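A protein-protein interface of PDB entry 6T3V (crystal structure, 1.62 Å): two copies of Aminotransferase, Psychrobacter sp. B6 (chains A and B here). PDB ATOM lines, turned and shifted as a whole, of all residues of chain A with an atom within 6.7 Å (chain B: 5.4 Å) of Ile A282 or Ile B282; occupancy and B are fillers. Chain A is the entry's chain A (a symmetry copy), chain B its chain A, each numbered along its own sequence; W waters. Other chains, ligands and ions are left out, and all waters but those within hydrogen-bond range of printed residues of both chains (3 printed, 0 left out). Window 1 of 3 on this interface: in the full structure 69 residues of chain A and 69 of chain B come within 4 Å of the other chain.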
ATOM      1  N   ILE A 101      -1.646  -9.443 -21.640  1.00  0.00           N
ATOM      2  CA  ILE A 101      -0.324  -9.093 -22.213  1.00  0.00           C
ATOM      3  C   ILE A 101       0.176 -10.374 -22.923  1.00  0.00           C
ATOM      4  O   ILE A 101       0.977 -11.160 -22.339  1.00  0.00           O
ATOM      5  CB  ILE A 101       0.634  -8.692 -21.075  1.00  0.00           C
ATOM      6  CG1 ILE A 101      -0.016  -7.646 -20.157  1.00  0.00           C
ATOM      7  CG2 ILE A 101       1.937  -8.159 -21.659  1.00  0.00           C
ATOM      8  CD1 ILE A 101      -0.448  -6.384 -20.898  1.00  0.00           C
ATOM      9  N   SER A 104       1.272 -15.239 -22.536  1.00  0.00           N
ATOM     10  CA  SER A 104       2.062 -15.309 -21.279  1.00  0.00           C
ATOM     11  C   SER A 104       1.344 -14.567 -20.171  1.00  0.00           C
ATOM     12  O   SER A 104       1.180 -15.083 -19.057  1.00  0.00           O
ATOM     13  CB  SER A 104       3.493 -14.718 -21.449  1.00  0.00           C
ATOM     14  OG  SER A 104       4.194 -15.490 -22.410  1.00  0.00           O
ATOM     15  N   GLY A 105       0.912 -13.340 -20.469  1.00  0.00           N
ATOM     16  CA  GLY A 105       0.184 -12.568 -19.426  1.00  0.00           C
ATOM     17  C   GLY A 105      -1.157 -13.190 -19.050  1.00  0.00           C
ATOM     18  O   GLY A 105      -1.608 -13.036 -17.908  1.00  0.00           O
ATOM     19  N   ALA A 106      -1.841 -13.862 -20.000  1.00  0.00           N
ATOM     20  CA  ALA A 106      -3.069 -14.539 -19.640  1.00  0.00           C
ATOM     21  C   ALA A 106      -2.798 -15.705 -18.683  1.00  0.00           C
ATOM     22  O   ALA A 106      -3.557 -15.906 -17.713  1.00  0.00           O
ATOM     23  CB  ALA A 106      -3.736 -15.083 -20.922  1.00  0.00           C
ATOM     24  N   LEU A 107      -1.773 -16.494 -19.000  1.00  0.00           N
ATOM     25  CA  LEU A 107      -1.391 -17.612 -18.098  1.00  0.00           C
ATOM     26  C   LEU A 107      -1.051 -17.049 -16.698  1.00  0.00           C
ATOM     27  O   LEU A 107      -1.445 -17.628 -15.675  1.00  0.00           O
ATOM     28  CB  LEU A 107      -0.169 -18.354 -18.673  1.00  0.00           C
ATOM     29  CG  LEU A 107      -0.534 -19.211 -19.907  1.00  0.00           C
ATOM     30  CD1 LEU A 107       0.747 -19.429 -20.770  1.00  0.00           C
ATOM     31  CD2 LEU A 107      -1.153 -20.559 -19.463  1.00  0.00           C
ATOM     32  N   LYS A 108      -0.303 -15.934 -16.642  1.00  0.00           N
ATOM     33  CA  LYS A 108       0.069 -15.348 -15.345  1.00  0.00           C
ATOM     34  C   LYS A 108      -1.164 -14.880 -14.571  1.00  0.00           C
ATOM     35  O   LYS A 108      -1.281 -15.147 -13.366  1.00  0.00           O
ATOM     36  CB  LYS A 108       1.037 -14.178 -15.560  1.00  0.00           C
ATOM     37  CG  LYS A 108       1.425 -13.416 -14.271  1.00  0.00           C
ATOM     38  CD  LYS A 108       2.169 -14.331 -13.281  1.00  0.00           C
ATOM     39  CE  LYS A 108       2.715 -13.397 -12.169  1.00  0.00           C
ATOM     40  NZ  LYS A 108       3.462 -14.181 -11.101  1.00  0.00           N
ATOM     41  N   VAL A 109      -2.079 -14.147 -15.213  1.00  0.00           N
ATOM     42  CA  VAL A 109      -3.289 -13.715 -14.467  1.00  0.00           C
ATOM     43  C   VAL A 109      -4.090 -14.949 -14.001  1.00  0.00           C
ATOM     44  O   VAL A 109      -4.563 -14.955 -12.865  1.00  0.00           O
ATOM     45  CB  VAL A 109      -4.166 -12.781 -15.342  1.00  0.00           C
ATOM     46  CG1 VAL A 109      -5.509 -12.490 -14.644  1.00  0.00           C
ATOM     47  CG2 VAL A 109      -3.403 -11.463 -15.602  1.00  0.00           C
ATOM     48  N   GLU A 112      -2.283 -16.470 -11.073  1.00  0.00           N
ATOM     49  CA  GLU A 112      -2.449 -15.645  -9.856  1.00  0.00           C
ATOM     50  C   GLU A 112      -3.855 -15.820  -9.245  1.00  0.00           C
ATOM     51  O   GLU A 112      -4.001 -15.931  -8.010  1.00  0.00           O
ATOM     52  CB  GLU A 112      -2.163 -14.175 -10.138  1.00  0.00           C
ATOM     53  CG  GLU A 112      -0.697 -13.866 -10.406  1.00  0.00           C
ATOM     54  CD  GLU A 112      -0.036 -13.082  -9.290  1.00  0.00           C
ATOM     55  OE1 GLU A 112      -0.579 -13.057  -8.157  1.00  0.00           O
ATOM     56  OE2 GLU A 112       1.070 -12.531  -9.513  1.00  0.00           O
ATOM     57  N   ASN A 132       7.960 -22.257 -20.416  1.00  0.00           N
ATOM     58  CA  ASN A 132       7.437 -21.128 -19.648  1.00  0.00           C
ATOM     59  C   ASN A 132       6.117 -21.431 -18.913  1.00  0.00           C
ATOM     60  O   ASN A 132       5.753 -20.705 -17.988  1.00  0.00           O
ATOM     61  CB  ASN A 132       7.281 -19.897 -20.574  1.00  0.00           C
ATOM     62  CG  ASN A 132       7.498 -18.574 -19.832  1.00  0.00           C
ATOM     63  OD1 ASN A 132       8.264 -18.527 -18.873  1.00  0.00           O
ATOM     64  ND2 ASN A 132       6.846 -17.477 -20.299  1.00  0.00           N
ATOM     65  N   ALA A 135       7.448 -22.156 -15.574  1.00  0.00           N
ATOM     66  CA  ALA A 135       8.023 -20.935 -14.963  1.00  0.00           C
ATOM     67  C   ALA A 135       6.913 -19.994 -14.464  1.00  0.00           C
ATOM     68  O   ALA A 135       6.994 -19.434 -13.368  1.00  0.00           O
ATOM     69  CB  ALA A 135       9.031 -20.224 -15.915  1.00  0.00           C
ATOM     70  N   ILE A 136       5.851 -19.836 -15.267  1.00  0.00           N
ATOM     71  CA  ILE A 136       4.790 -18.896 -14.893  1.00  0.00           C
ATOM     72  C   ILE A 136       4.037 -19.415 -13.643  1.00  0.00           C
ATOM     73  O   ILE A 136       3.839 -18.677 -12.679  1.00  0.00           O
ATOM     74  CB  ILE A 136       3.794 -18.710 -16.079  1.00  0.00           C
ATOM     75  CG1 ILE A 136       4.504 -17.924 -17.185  1.00  0.00           C
ATOM     76  CG2 ILE A 136       2.539 -17.968 -15.598  1.00  0.00           C
ATOM     77  CD1 ILE A 136       3.715 -17.966 -18.521  1.00  0.00           C
ATOM     78  N   SER A 277      -9.358  -7.244 -10.450  1.00  0.00           N
ATOM     79  CA  SER A 277      -8.507  -7.004  -9.280  1.00  0.00           C
ATOM     80  C   SER A 277      -7.081  -7.566  -9.488  1.00  0.00           C
ATOM     81  O   SER A 277      -6.076  -6.938  -9.122  1.00  0.00           O
ATOM     82  CB  SER A 277      -9.137  -7.704  -8.076  1.00  0.00           C
ATOM     83  OG  SER A 277      -8.296  -7.546  -6.938  1.00  0.00           O
ATOM     84  N   THR A 278      -7.002  -8.749 -10.111  1.00  0.00           N
ATOM     85  CA  THR A 278      -5.718  -9.411 -10.337  1.00  0.00           C
ATOM     86  C   THR A 278      -4.880  -8.595 -11.323  1.00  0.00           C
ATOM     87  O   THR A 278      -3.697  -8.315 -11.063  1.00  0.00           O
ATOM     88  CB  THR A 278      -5.942 -10.865 -10.820  1.00  0.00           C
ATOM     89  OG1 THR A 278      -6.709 -11.541  -9.814  1.00  0.00           O
ATOM     90  CG2 THR A 278      -4.613 -11.604 -10.968  1.00  0.00           C
ATOM     91  N   VAL A 279      -5.495  -8.165 -12.433  1.00  0.00           N
ATOM     92  CA  VAL A 279      -4.817  -7.278 -13.394  1.00  0.00           C
ATOM     93  C   VAL A 279      -4.279  -6.027 -12.696  1.00  0.00           C
ATOM     94  O   VAL A 279      -3.137  -5.618 -12.931  1.00  0.00           O
ATOM     95  CB  VAL A 279      -5.754  -6.875 -14.549  1.00  0.00           C
ATOM     96  CG1 VAL A 279      -5.160  -5.717 -15.355  1.00  0.00           C
ATOM     97  CG2 VAL A 279      -6.009  -8.076 -15.477  1.00  0.00           C
ATOM     98  N   ARG A 280      -5.119  -5.419 -11.865  1.00  0.00           N
ATOM     99  CA  ARG A 280      -4.779  -4.111 -11.265  1.00  0.00           C
ATOM    100  C   ARG A 280      -3.453  -4.239 -10.521  1.00  0.00           C
ATOM    101  O   ARG A 280      -2.651  -3.307 -10.619  1.00  0.00           O
ATOM    102  CB  ARG A 280      -5.906  -3.680 -10.320  1.00  0.00           C
ATOM    103  CG  ARG A 280      -5.608  -2.388  -9.548  1.00  0.00           C
ATOM    104  CD  ARG A 280      -5.299  -1.192 -10.441  1.00  0.00           C
ATOM    105  NE  ARG A 280      -5.505   0.062  -9.644  1.00  0.00           N
ATOM    106  CZ  ARG A 280      -5.027   1.254 -10.009  1.00  0.00           C
ATOM    107  NH1 ARG A 280      -4.216   1.388 -11.059  1.00  0.00           N
ATOM    108  NH2 ARG A 280      -5.295   2.322  -9.239  1.00  0.00           N
ATOM    109  N   ARG A 281      -3.239  -5.356  -9.800  1.00  0.00           N
ATOM    110  CA  ARG A 281      -2.033  -5.514  -8.969  1.00  0.00           C
ATOM    111  C   ARG A 281      -0.855  -6.165  -9.689  1.00  0.00           C
ATOM    112  O   ARG A 281       0.167  -6.460  -9.058  1.00  0.00           O
ATOM    113  CB  ARG A 281      -2.376  -6.293  -7.691  1.00  0.00           C
ATOM    114  CG  ARG A 281      -2.784  -7.723  -7.950  1.00  0.00           C
ATOM    115  CD  ARG A 281      -2.991  -8.379  -6.588  1.00  0.00           C
ATOM    116  NE  ARG A 281      -3.506  -9.726  -6.765  1.00  0.00           N
ATOM    117  CZ  ARG A 281      -2.769 -10.766  -7.086  1.00  0.00           C
ATOM    118  NH1 ARG A 281      -1.437 -10.624  -7.253  1.00  0.00           N
ATOM    119  NH2 ARG A 281      -3.352 -12.000  -7.156  1.00  0.00           N
ATOM    120  N   ILE A 282      -0.956  -6.359 -11.028  1.00  0.00           N
ATOM    121  CA  ILE A 282       0.167  -6.857 -11.820  1.00  0.00           C
ATOM    122  C   ILE A 282       0.671  -5.782 -12.777  1.00  0.00           C
ATOM    123  O   ILE A 282       1.863  -5.453 -12.800  1.00  0.00           O
ATOM    124  CB  ILE A 282      -0.214  -8.136 -12.605  1.00  0.00           C
ATOM    125  CG1 ILE A 282      -0.685  -9.214 -11.616  1.00  0.00           C
ATOM    126  CG2 ILE A 282       1.014  -8.642 -13.399  1.00  0.00           C
ATOM    127  CD1 ILE A 282      -1.190 -10.484 -12.323  1.00  0.00           C
ATOM    128  N   TYR A 283      -0.264  -5.165 -13.510  1.00  0.00           N
ATOM    129  CA  TYR A 283       0.147  -4.134 -14.519  1.00  0.00           C
ATOM    130  C   TYR A 283      -0.898  -3.060 -14.763  1.00  0.00           C
ATOM    131  O   TYR A 283      -0.700  -2.253 -15.679  1.00  0.00           O
ATOM    132  CB  TYR A 283       0.612  -4.743 -15.890  1.00  0.00           C
ATOM    133  CG  TYR A 283      -0.453  -5.615 -16.465  1.00  0.00           C
ATOM    134  CD1 TYR A 283      -0.493  -6.990 -16.161  1.00  0.00           C
ATOM    135  CD2 TYR A 283      -1.461  -5.072 -17.308  1.00  0.00           C
ATOM    136  CE1 TYR A 283      -1.538  -7.802 -16.654  1.00  0.00           C
ATOM    137  CE2 TYR A 283      -2.477  -5.879 -17.789  1.00  0.00           C
ATOM    138  CZ  TYR A 283      -2.518  -7.243 -17.476  1.00  0.00           C
ATOM    139  OH  TYR A 283      -3.555  -8.025 -17.953  1.00  0.00           O
ATOM    140  N   SER A 284      -1.969  -3.044 -13.969  1.00  0.00           N
ATOM    141  CA  SER A 284      -3.022  -2.006 -14.008  1.00  0.00           C
ATOM    142  C   SER A 284      -3.999  -2.139 -15.180  1.00  0.00           C
ATOM    143  O   SER A 284      -5.214  -2.263 -14.958  1.00  0.00           O
ATOM    144  CB  SER A 284      -2.422  -0.588 -13.929  1.00  0.00           C
ATOM    145  OG  SER A 284      -3.432   0.314 -13.578  1.00  0.00           O
ATOM    146  N   SER A 285      -3.489  -2.101 -16.416  1.00  0.00           N
ATOM    147  CA  SER A 285      -4.368  -2.249 -17.601  1.00  0.00           C
ATOM    148  C   SER A 285      -3.463  -2.546 -18.803  1.00  0.00           C
ATOM    149  O   SER A 285      -2.262  -2.259 -18.785  1.00  0.00           O
ATOM    150  CB  SER A 285      -5.222  -0.974 -17.834  1.00  0.00           C
ATOM    151  OG  SER A 285      -4.381   0.189 -17.879  1.00  0.00           O
ATOM    152  N   SER B 104       3.202   0.548 -12.734  1.00  0.00           N
ATOM    153  CA  SER B 104       2.588  -0.615 -12.041  1.00  0.00           C
ATOM    154  C   SER B 104       3.380  -1.873 -12.333  1.00  0.00           C
ATOM    155  O   SER B 104       3.726  -2.636 -11.422  1.00  0.00           O
ATOM    156  CB  SER B 104       1.103  -0.834 -12.460  1.00  0.00           C
ATOM    157  OG  SER B 104       0.350   0.306 -12.080  1.00  0.00           O
ATOM    158  N   GLY B 105       3.669  -2.101 -13.616  1.00  0.00           N
ATOM    159  CA  GLY B 105       4.459  -3.312 -13.963  1.00  0.00           C
ATOM    160  C   GLY B 105       5.884  -3.273 -13.418  1.00  0.00           C
ATOM    161  O   GLY B 105       6.464  -4.328 -13.134  1.00  0.00           O
ATOM    162  N   LYS B 108       5.571  -4.317  -9.830  1.00  0.00           N
ATOM    163  CA  LYS B 108       5.321  -5.765  -9.764  1.00  0.00           C
ATOM    164  C   LYS B 108       6.603  -6.563 -10.016  1.00  0.00           C
ATOM    165  O   LYS B 108       6.894  -7.520  -9.284  1.00  0.00           O
ATOM    166  CB  LYS B 108       4.242  -6.157 -10.780  1.00  0.00           C
ATOM    167  CG  LYS B 108       3.962  -7.675 -10.872  1.00  0.00           C
ATOM    168  CD  LYS B 108       3.429  -8.228  -9.539  1.00  0.00           C
ATOM    169  CE  LYS B 108       2.955  -9.675  -9.839  1.00  0.00           C
ATOM    170  NZ  LYS B 108       2.418 -10.356  -8.589  1.00  0.00           N
ATOM    171  N   VAL B 109       7.365  -6.230 -11.062  1.00  0.00           N
ATOM    172  CA  VAL B 109       8.621  -6.988 -11.290  1.00  0.00           C
ATOM    173  C   VAL B 109       9.572  -6.807 -10.089  1.00  0.00           C
ATOM    174  O   VAL B 109      10.186  -7.787  -9.666  1.00  0.00           O
ATOM    175  CB  VAL B 109       9.300  -6.535 -12.609  1.00  0.00           C
ATOM    176  CG1 VAL B 109      10.694  -7.179 -12.749  1.00  0.00           C
ATOM    177  CG2 VAL B 109       8.406  -6.933 -13.805  1.00  0.00           C
ATOM    178  N   GLU B 112       8.285  -8.926  -7.258  1.00  0.00           N
ATOM    179  CA  GLU B 112       8.538 -10.362  -7.509  1.00  0.00           C
ATOM    180  C   GLU B 112      10.021 -10.721  -7.274  1.00  0.00           C
ATOM    181  O   GLU B 112      10.332 -11.770  -6.674  1.00  0.00           O
ATOM    182  CB  GLU B 112       8.101 -10.767  -8.910  1.00  0.00           C
ATOM    183  CG  GLU B 112       6.592 -10.779  -9.112  1.00  0.00           C
ATOM    184  CD  GLU B 112       6.018 -12.174  -9.262  1.00  0.00           C
ATOM    185  OE1 GLU B 112       6.698 -13.159  -8.877  1.00  0.00           O
ATOM    186  OE2 GLU B 112       4.852 -12.301  -9.710  1.00  0.00           O
ATOM    187  N   ILE B 136      -0.020  -4.362  -4.959  1.00  0.00           N
ATOM    188  CA  ILE B 136       1.000  -5.019  -5.782  1.00  0.00           C
ATOM    189  C   ILE B 136       1.948  -5.856  -4.885  1.00  0.00           C
ATOM    190  O   ILE B 136       2.207  -7.025  -5.168  1.00  0.00           O
ATOM    191  CB  ILE B 136       1.818  -3.953  -6.576  1.00  0.00           C
ATOM    192  CG1 ILE B 136       0.911  -3.358  -7.656  1.00  0.00           C
ATOM    193  CG2 ILE B 136       3.060  -4.605  -7.201  1.00  0.00           C
ATOM    194  CD1 ILE B 136       1.523  -2.076  -8.282  1.00  0.00           C
ATOM    195  N   THR B 278      12.447 -12.747 -14.391  1.00  0.00           N
ATOM    196  CA  THR B 278      11.204 -12.361 -13.729  1.00  0.00           C
ATOM    197  C   THR B 278      10.182 -11.897 -14.768  1.00  0.00           C
ATOM    198  O   THR B 278       9.023 -12.348 -14.759  1.00  0.00           O
ATOM    199  CB  THR B 278      11.480 -11.281 -12.654  1.00  0.00           C
ATOM    200  OG1 THR B 278      12.421 -11.829 -11.722  1.00  0.00           O
ATOM    201  CG2 THR B 278      10.208 -10.936 -11.882  1.00  0.00           C
ATOM    202  N   VAL B 279      10.613 -11.036 -15.700  1.00  0.00           N
ATOM    203  CA  VAL B 279       9.747 -10.612 -16.814  1.00  0.00           C
ATOM    204  C   VAL B 279       9.205 -11.823 -17.575  1.00  0.00           C
ATOM    205  O   VAL B 279       8.011 -11.882 -17.896  1.00  0.00           O
ATOM    206  CB  VAL B 279      10.493  -9.673 -17.783  1.00  0.00           C
ATOM    207  CG1 VAL B 279       9.709  -9.499 -19.086  1.00  0.00           C
ATOM    208  CG2 VAL B 279      10.724  -8.300 -17.128  1.00  0.00           C
ATOM    209  N   ARG B 280      10.091 -12.765 -17.879  1.00  0.00           N
ATOM    210  CA  ARG B 280       9.726 -13.897 -18.757  1.00  0.00           C
ATOM    211  C   ARG B 280       8.521 -14.616 -18.159  1.00  0.00           C
ATOM    212  O   ARG B 280       7.641 -14.997 -18.934  1.00  0.00           O
ATOM    213  CB  ARG B 280      10.927 -14.841 -18.890  1.00  0.00           C
ATOM    214  CG  ARG B 280      10.626 -16.116 -19.688  1.00  0.00           C
ATOM    215  CD  ARG B 280      10.110 -15.857 -21.099  1.00  0.00           C
ATOM    216  NE  ARG B 280      10.314 -17.098 -21.916  1.00  0.00           N
ATOM    217  CZ  ARG B 280       9.698 -17.325 -23.078  1.00  0.00           C
ATOM    218  NH1 ARG B 280       8.751 -16.506 -23.536  1.00  0.00           N
ATOM    219  NH2 ARG B 280       9.974 -18.457 -23.747  1.00  0.00           N
ATOM    220  N   ARG B 281       8.493 -14.799 -16.825  1.00  0.00           N
ATOM    221  CA  ARG B 281       7.421 -15.574 -16.179  1.00  0.00           C
ATOM    222  C   ARG B 281       6.216 -14.741 -15.746  1.00  0.00           C
ATOM    223  O   ARG B 281       5.311 -15.263 -15.086  1.00  0.00           O
ATOM    224  CB  ARG B 281       7.986 -16.357 -14.985  1.00  0.00           C
ATOM    225  CG  ARG B 281       8.471 -15.472 -13.863  1.00  0.00           C
ATOM    226  CD  ARG B 281       8.904 -16.396 -12.726  1.00  0.00           C
ATOM    227  NE  ARG B 281       9.499 -15.612 -11.658  1.00  0.00           N
ATOM    228  CZ  ARG B 281       8.814 -14.933 -10.764  1.00  0.00           C
ATOM    229  NH1 ARG B 281       7.465 -14.953 -10.792  1.00  0.00           N
ATOM    230  NH2 ARG B 281       9.482 -14.290  -9.761  1.00  0.00           N
ATOM    231  N   ILE B 282       6.161 -13.447 -16.149  1.00  0.00           N
ATOM    232  CA  ILE B 282       4.989 -12.612 -15.891  1.00  0.00           C
ATOM    233  C   ILE B 282       4.282 -12.258 -17.194  1.00  0.00           C
ATOM    234  O   ILE B 282       3.073 -12.476 -17.347  1.00  0.00           O
ATOM    235  CB  ILE B 282       5.368 -11.322 -15.122  1.00  0.00           C
ATOM    236  CG1 ILE B 282       6.048 -11.706 -13.797  1.00  0.00           C
ATOM    237  CG2 ILE B 282       4.094 -10.490 -14.844  1.00  0.00           C
ATOM    238  CD1 ILE B 282       6.559 -10.481 -13.020  1.00  0.00           C
ATOM    239  N   TYR B 283       5.061 -11.790 -18.178  1.00  0.00           N
ATOM    240  CA  TYR B 283       4.442 -11.364 -19.475  1.00  0.00           C
ATOM    241  C   TYR B 283       5.356 -11.525 -20.677  1.00  0.00           C
ATOM    242  O   TYR B 283       4.978 -11.067 -21.761  1.00  0.00           O
ATOM    243  CB  TYR B 283       3.856  -9.907 -19.446  1.00  0.00           C
ATOM    244  CG  TYR B 283       4.905  -8.927 -19.041  1.00  0.00           C
ATOM    245  CD1 TYR B 283       5.096  -8.602 -17.684  1.00  0.00           C
ATOM    246  CD2 TYR B 283       5.750  -8.324 -20.013  1.00  0.00           C
ATOM    247  CE1 TYR B 283       6.131  -7.724 -17.297  1.00  0.00           C
ATOM    248  CE2 TYR B 283       6.758  -7.460 -19.622  1.00  0.00           C
ATOM    249  CZ  TYR B 283       6.949  -7.148 -18.270  1.00  0.00           C
ATOM    250  OH  TYR B 283       7.977  -6.298 -17.902  1.00  0.00           O
ATOM    251  N   SER B 284       6.516 -12.158 -20.494  1.00  0.00           N
ATOM    252  CA  SER B 284       7.467 -12.487 -21.577  1.00  0.00           C
ATOM    253  C   SER B 284       8.294 -11.297 -22.076  1.00  0.00           C
ATOM    254  O   SER B 284       9.534 -11.345 -22.027  1.00  0.00           O
ATOM    255  CB  SER B 284       6.770 -13.219 -22.740  1.00  0.00           C
ATOM    256  OG  SER B 284       7.740 -13.843 -23.532  1.00  0.00           O
HETATM  257  O   HOH W   1       5.175 -16.138 -12.534  1.00  0.00           O
HETATM  258  O   HOH W   2       9.617 -21.747 -22.761  1.00  0.00           O
HETATM  259  O   HOH W   3       0.698  -8.361  -7.216  1.00  0.00           O
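Gly A105 touches Ile B282, and with the chains exchanged Ile A282 touches Gly B105. Lys A108 touches Arg B281, and with the chains exchanged Arg A281 touches Lys B108. Glu A112 touches its own counterpart, Glu B112. Ile B282 touches its own counterpart, Ile A282. 13 positions are printed for both chains.
Ile A101 touches Tyr B283 (CG2 to CB, 3.4 Å). Ser A104 touches Ile B282. Ser B284 touches Ser A104 (CB to OG, 3.4 Å). Glu A112 touches Glu B112. O of Arg B281 touches CG1 of Ile A136, at 3.5 Å. Arg A281 touches Ile B136. Ser B104 touches Ile A282. Ile A282 touches Gly B105. Ile A282 touches Lys B108 (O to CB, 3.2 Å). Ser B104 touches Ser A284.
Of the 20 printed residues of chain A, 12 touch a printed residue of chain B. Hydrophobic or aromatic side chains of chain A within 4 Å of the printed part of chain B: Ile A101, Ile A136 and Ile A282. Of the 13 printed residues of chain B, 10 touch a printed residue of chain A. Hydrophobic or aromatic side chains of chain B that line the printed part of chain A: Ile B136, Ile B282 and Tyr B283. Among the printed residues, 21 pairs touch across the chains.
The side-chain amino group (NZ) of Lys B108 lies within salt-bridge range of the side-chain carboxylate (OE2) of Glu B112 (3.3 Å). OE1 of Glu B112 lies within salt-bridge range of NH1 of Arg B281 (2.7 Å). The backbone NH (N) of Ser B284 sits at hydrogen-bond distance from the backbone carbonyl oxygen (O) of Val B279, 3.0 Å away. NZ of Lys A108 is in salt-bridge range of OE2 of Glu A112. N of Ser A284 lies within hydrogen-bond range of O of Val A279 (3.0 Å). The guanidinium group of Arg A280 is in hydrogen-bond range of the side-chain hydroxyl of Ser A284 (2.8 Å).
Of chain B, only Ser B104 (3.6 Å), Gly B105 (3.6 Å), Lys B108 (3.2 Å) and Ile B282 (3.9 Å) come within 4 Å of Ile A282. Ile B282 touches just these residues of chain A: Ser A104 (3.6 Å), Gly A105 (3.6 Å), Lys A108 (3.2 Å) and Ile A282 (3.9 Å). Printed residues of chain A within 4 Å of Lys B108: Glu A112, Arg A281 and Ile A282. Printed residues of chain A within 4 Å of Ser B284: Ser A104. Of the printed residues of chain A, Ile B136 touches Arg A281. Of the printed residues of chain B, Ile A136 touches Arg B281. Of the printed residues of chain B, Glu A112 touches Lys B108 (2.7 Å) and Glu B112 (3.8 Å).
Water W3 lies within hydrogen-bond range of O of Arg A281, O of Ile B136 and NZ of Lys B108. Water W1 lies within hydrogen-bond range of O of Arg B281 (2.7 Å), O of Ile A136 (2.9 Å) and NZ of Lys A108 (3.0 Å). Water W2 lies within hydrogen-bond range of the backbone NH (N) of Asn A132 (2.9 Å) and the guanidinium group (NH2) of Arg B280 (3.5 Å).
NZ of Lys B108 lies within salt-bridge range of OE2 of Glu A112, 2.7 Å away. The side-chain carboxylate (OE2) of Glu B112 lies within salt-bridge range of the side-chain amino group (NZ) of Lys A108, 2.7 Å away. ND2 of Asn A132 sits at hydrogen-bond distance from O of Arg B280 (2.9 Å).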
